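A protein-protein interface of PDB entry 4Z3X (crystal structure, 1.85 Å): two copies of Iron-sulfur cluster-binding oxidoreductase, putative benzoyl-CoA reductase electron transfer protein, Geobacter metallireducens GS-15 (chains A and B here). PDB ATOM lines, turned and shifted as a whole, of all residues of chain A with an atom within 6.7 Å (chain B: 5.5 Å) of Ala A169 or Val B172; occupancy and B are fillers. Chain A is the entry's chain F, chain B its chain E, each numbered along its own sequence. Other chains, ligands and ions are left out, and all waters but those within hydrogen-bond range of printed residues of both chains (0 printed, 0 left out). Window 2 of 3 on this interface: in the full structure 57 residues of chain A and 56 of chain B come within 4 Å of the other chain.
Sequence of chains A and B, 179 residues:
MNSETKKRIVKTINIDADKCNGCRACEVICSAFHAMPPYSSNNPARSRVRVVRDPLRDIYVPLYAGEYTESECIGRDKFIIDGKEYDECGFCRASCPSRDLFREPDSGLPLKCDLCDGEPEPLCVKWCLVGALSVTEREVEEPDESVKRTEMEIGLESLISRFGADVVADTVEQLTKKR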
ATOM      1  N   LEU A 156      27.741  22.340  22.351  1.00  0.00           N
ATOM      2  CA  LEU A 156      26.547  23.141  22.632  1.00  0.00           C
ATOM      3  C   LEU A 156      25.279  22.393  22.269  1.00  0.00           C
ATOM      4  O   LEU A 156      24.308  22.370  23.062  1.00  0.00           O
ATOM      5  CB  LEU A 156      26.561  24.463  21.863  1.00  0.00           C
ATOM      6  CG  LEU A 156      27.012  25.797  22.455  1.00  0.00           C
ATOM      7  CD1 LEU A 156      26.825  25.892  23.982  1.00  0.00           C
ATOM      8  CD2 LEU A 156      28.431  26.058  22.029  1.00  0.00           C
ATOM      9  N   ILE A 160      22.000  21.599  24.412  1.00  0.00           N
ATOM     10  CA  ILE A 160      20.662  21.958  23.996  1.00  0.00           C
ATOM     11  C   ILE A 160      19.725  20.712  23.953  1.00  0.00           C
ATOM     12  O   ILE A 160      18.566  20.813  24.348  1.00  0.00           O
ATOM     13  CB  ILE A 160      20.702  22.664  22.627  1.00  0.00           C
ATOM     14  CG1 ILE A 160      21.346  24.044  22.807  1.00  0.00           C
ATOM     15  CG2 ILE A 160      19.292  22.776  22.029  1.00  0.00           C
ATOM     16  CD1 ILE A 160      21.369  24.830  21.552  1.00  0.00           C
ATOM     17  N   GLY A 164      17.466  21.925  26.651  1.00  0.00           N
ATOM     18  CA  GLY A 164      16.528  22.875  26.055  1.00  0.00           C
ATOM     19  C   GLY A 164      17.197  24.129  25.512  1.00  0.00           C
ATOM     20  O   GLY A 164      18.061  24.701  26.169  1.00  0.00           O
ATOM     21  N   ALA A 165      16.800  24.546  24.308  1.00  0.00           N
ATOM     22  CA  ALA A 165      17.396  25.699  23.618  1.00  0.00           C
ATOM     23  C   ALA A 165      17.263  27.002  24.416  1.00  0.00           C
ATOM     24  O   ALA A 165      18.233  27.749  24.552  1.00  0.00           O
ATOM     25  CB  ALA A 165      16.775  25.858  22.219  1.00  0.00           C
ATOM     26  N   ASP A 166      16.073  27.252  24.963  1.00  0.00           N
ATOM     27  CA  ASP A 166      15.814  28.448  25.786  1.00  0.00           C
ATOM     28  C   ASP A 166      16.562  28.445  27.127  1.00  0.00           C
ATOM     29  O   ASP A 166      17.146  29.445  27.504  1.00  0.00           O
ATOM     30  CB  ASP A 166      14.294  28.637  26.023  1.00  0.00           C
ATOM     31  CG  ASP A 166      13.592  27.386  26.570  1.00  0.00           C
ATOM     32  OD1 ASP A 166      13.915  26.248  26.138  1.00  0.00           O
ATOM     33  OD2 ASP A 166      12.686  27.564  27.423  1.00  0.00           O
ATOM     34  N   VAL A 167      16.545  27.323  27.837  1.00  0.00           N
ATOM     35  CA  VAL A 167      17.371  27.131  29.030  1.00  0.00           C
ATOM     36  C   VAL A 167      18.844  27.403  28.762  1.00  0.00           C
ATOM     37  O   VAL A 167      19.488  28.171  29.494  1.00  0.00           O
ATOM     38  CB  VAL A 167      17.222  25.682  29.563  1.00  0.00           C
ATOM     39  CG1 VAL A 167      18.006  25.487  30.842  1.00  0.00           C
ATOM     40  CG2 VAL A 167      15.773  25.379  29.777  1.00  0.00           C
ATOM     41  N   VAL A 168      19.389  26.768  27.720  1.00  0.00           N
ATOM     42  CA  VAL A 168      20.811  26.928  27.436  1.00  0.00           C
ATOM     43  C   VAL A 168      21.116  28.407  27.092  1.00  0.00           C
ATOM     44  O   VAL A 168      22.044  28.993  27.654  1.00  0.00           O
ATOM     45  CB  VAL A 168      21.265  25.985  26.320  1.00  0.00           C
ATOM     46  CG1 VAL A 168      22.564  26.481  25.659  1.00  0.00           C
ATOM     47  CG2 VAL A 168      21.348  24.478  26.831  1.00  0.00           C
ATOM     48  N   ALA A 169      20.301  29.017  26.232  1.00  0.00           N
ATOM     49  CA  ALA A 169      20.541  30.379  25.734  1.00  0.00           C
ATOM     50  C   ALA A 169      20.503  31.401  26.862  1.00  0.00           C
ATOM     51  O   ALA A 169      21.265  32.367  26.885  1.00  0.00           O
ATOM     52  CB  ALA A 169      19.505  30.751  24.674  1.00  0.00           C
ATOM     53  N   ASP A 170      19.589  31.168  27.787  1.00  0.00           N
ATOM     54  CA  ASP A 170      19.375  32.023  28.926  1.00  0.00           C
ATOM     55  C   ASP A 170      20.533  31.948  29.898  1.00  0.00           C
ATOM     56  O   ASP A 170      21.050  32.985  30.336  1.00  0.00           O
ATOM     57  CB  ASP A 170      18.073  31.644  29.618  1.00  0.00           C
ATOM     58  CG  ASP A 170      16.869  32.223  28.921  1.00  0.00           C
ATOM     59  OD1 ASP A 170      17.024  33.285  28.281  1.00  0.00           O
ATOM     60  OD2 ASP A 170      15.768  31.641  29.025  1.00  0.00           O
ATOM     61  N   THR A 171      20.937  30.728  30.227  1.00  0.00           N
ATOM     62  CA  THR A 171      22.111  30.498  31.049  1.00  0.00           C
ATOM     63  C   THR A 171      23.335  31.148  30.397  1.00  0.00           C
ATOM     64  O   THR A 171      24.209  31.681  31.088  1.00  0.00           O
ATOM     65  CB  THR A 171      22.372  28.985  31.276  1.00  0.00           C
ATOM     66  OG1 THR A 171      21.188  28.355  31.782  1.00  0.00           O
ATOM     67  CG2 THR A 171      23.519  28.762  32.271  1.00  0.00           C
ATOM     68  N   VAL A 172      23.402  31.129  29.070  1.00  0.00           N
ATOM     69  CA  VAL A 172      24.588  31.670  28.411  1.00  0.00           C
ATOM     70  C   VAL A 172      24.632  33.202  28.509  1.00  0.00           C
ATOM     71  O   VAL A 172      25.703  33.779  28.684  1.00  0.00           O
ATOM     72  CB  VAL A 172      24.678  31.245  26.921  1.00  0.00           C
ATOM     73  CG1 VAL A 172      25.671  32.153  26.137  1.00  0.00           C
ATOM     74  CG2 VAL A 172      25.086  29.760  26.799  1.00  0.00           C
ATOM     75  N   GLU A 173      23.468  33.836  28.367  1.00  0.00           N
ATOM     76  CA  GLU A 173      23.358  35.277  28.448  1.00  0.00           C
ATOM     77  C   GLU A 173      23.747  35.715  29.872  1.00  0.00           C
ATOM     78  O   GLU A 173      24.446  36.709  30.060  1.00  0.00           O
ATOM     79  CB  GLU A 173      21.930  35.723  28.074  1.00  0.00           C
ATOM     80  N   GLN A 174      23.312  34.935  30.861  1.00  0.00           N
ATOM     81  CA  GLN A 174      23.596  35.188  32.273  1.00  0.00           C
ATOM     82  C   GLN A 174      25.057  34.907  32.627  1.00  0.00           C
ATOM     83  O   GLN A 174      25.500  35.199  33.722  1.00  0.00           O
ATOM     84  CB  GLN A 174      22.662  34.352  33.162  1.00  0.00           C
ATOM     85  N   VAL B 167      32.850  33.783  21.381  1.00  0.00           N
ATOM     86  CA  VAL B 167      32.618  32.691  20.438  1.00  0.00           C
ATOM     87  C   VAL B 167      31.392  31.822  20.859  1.00  0.00           C
ATOM     88  O   VAL B 167      30.546  31.488  20.007  1.00  0.00           O
ATOM     89  CB  VAL B 167      33.890  31.816  20.285  1.00  0.00           C
ATOM     90  N   VAL B 168      31.288  31.481  22.158  1.00  0.00           N
ATOM     91  CA  VAL B 168      30.148  30.712  22.686  1.00  0.00           C
ATOM     92  C   VAL B 168      28.824  31.475  22.563  1.00  0.00           C
ATOM     93  O   VAL B 168      27.830  30.908  22.105  1.00  0.00           O
ATOM     94  CB  VAL B 168      30.315  30.311  24.149  1.00  0.00           C
ATOM     95  CG1 VAL B 168      29.076  29.574  24.610  1.00  0.00           C
ATOM     96  CG2 VAL B 168      31.552  29.438  24.345  1.00  0.00           C
ATOM     97  N   ALA B 169      28.808  32.756  22.944  1.00  0.00           N
ATOM     98  CA  ALA B 169      27.584  33.555  22.843  1.00  0.00           C
ATOM     99  C   ALA B 169      27.023  33.669  21.418  1.00  0.00           C
ATOM    100  O   ALA B 169      25.821  33.439  21.199  1.00  0.00           O
ATOM    101  CB  ALA B 169      27.834  34.958  23.417  1.00  0.00           C
ATOM    102  N   ASP B 170      27.872  34.032  20.450  1.00  0.00           N
ATOM    103  CA  ASP B 170      27.417  34.176  19.056  1.00  0.00           C
ATOM    104  C   ASP B 170      26.981  32.826  18.476  1.00  0.00           C
ATOM    105  O   ASP B 170      26.091  32.747  17.617  1.00  0.00           O
ATOM    106  CB  ASP B 170      28.513  34.801  18.181  1.00  0.00           C
ATOM    107  N   THR B 171      27.608  31.762  18.954  1.00  0.00           N
ATOM    108  CA  THR B 171      27.268  30.432  18.483  1.00  0.00           C
ATOM    109  C   THR B 171      25.896  30.005  18.993  1.00  0.00           C
ATOM    110  O   THR B 171      25.079  29.518  18.223  1.00  0.00           O
ATOM    111  CB  THR B 171      28.340  29.426  18.893  1.00  0.00           C
ATOM    112  OG1 THR B 171      29.389  29.455  17.920  1.00  0.00           O
ATOM    113  CG2 THR B 171      27.780  28.012  18.958  1.00  0.00           C
ATOM    114  N   VAL B 172      25.623  30.205  20.280  1.00  0.00           N
ATOM    115  CA  VAL B 172      24.329  29.797  20.848  1.00  0.00           C
ATOM    116  C   VAL B 172      23.181  30.518  20.099  1.00  0.00           C
ATOM    117  O   VAL B 172      22.090  29.977  19.951  1.00  0.00           O
ATOM    118  CB  VAL B 172      24.278  30.058  22.407  1.00  0.00           C
ATOM    119  CG1 VAL B 172      22.988  29.577  23.011  1.00  0.00           C
ATOM    120  CG2 VAL B 172      25.400  29.323  23.081  1.00  0.00           C
ATOM    121  N   GLU B 173      23.452  31.718  19.586  1.00  0.00           N
ATOM    122  CA  GLU B 173      22.480  32.435  18.755  1.00  0.00           C
ATOM    123  C   GLU B 173      22.507  31.979  17.270  1.00  0.00           C
ATOM    124  O   GLU B 173      22.911  32.724  16.370  1.00  0.00           O
ATOM    125  CB  GLU B 173      22.718  33.949  18.865  1.00  0.00           C
ATOM    126  N   GLN B 174      22.058  30.749  17.029  1.00  0.00           N
ATOM    127  CA  GLN B 174      22.016  30.170  15.685  1.00  0.00           C
ATOM    128  C   GLN B 174      21.760  28.679  15.812  1.00  0.00           C
ATOM    129  O   GLN B 174      21.987  28.096  16.883  1.00  0.00           O
ATOM    130  CB  GLN B 174      23.321  30.431  14.915  1.00  0.00           C
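O of Val B167 is in hydrogen-bond range of OG1 of Thr B171, 3.1 Å away.
Among the printed residues, pairs that only touch across the chains: Leu A156 with Thr B171 (3.7 Å), Ala A169 with Val B172 (3.7 Å), Val A172 with Val B172 (3.8 Å) and Leu A156 with Val B172 (3.8 Å).
Printed residues of chain B within 4 Å of Leu A156: Thr B171 (3.7 Å) and Val B172 (3.8 Å). Of the printed residues of chain B, Ala A169 touches Val B172. Printed residues of chain B within 4 Å of Val A172: Val B172 (3.8 Å). Of the printed residues of chain A, Thr B171 touches Leu A156 (3.7 Å). Val B172 touches three residues of chain A. Glu B173 touches none of the printed residues of chain A. The nearest printed residue of chain B that does not touch Ala A169 is Glu B173 (6.5 Å). The nearest printed residue of chain B that does not touch Val A172 is Ala B169 (4.1 Å).
Along chain A the printed residues that touch a printed residue of chain B span positions 156 to 172. Printed residues of chain B that touch a printed residue of chain A: Thr B171 and Val B172. Among the printed residues, 4 pairs touch across the chains.
Ala A169 touches Val B172, but with the chains exchanged Val A172 does not touch Ala B169 (4.1 Å). Val B172 touches its own counterpart, Val A172. Positions printed for both chains: 167, 168, 169, 170, 171, 172, 173 and 174. Of the 4 pairs that touch across the chains among the printed residues, 1 has its exchanged pair printed and touching as well.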
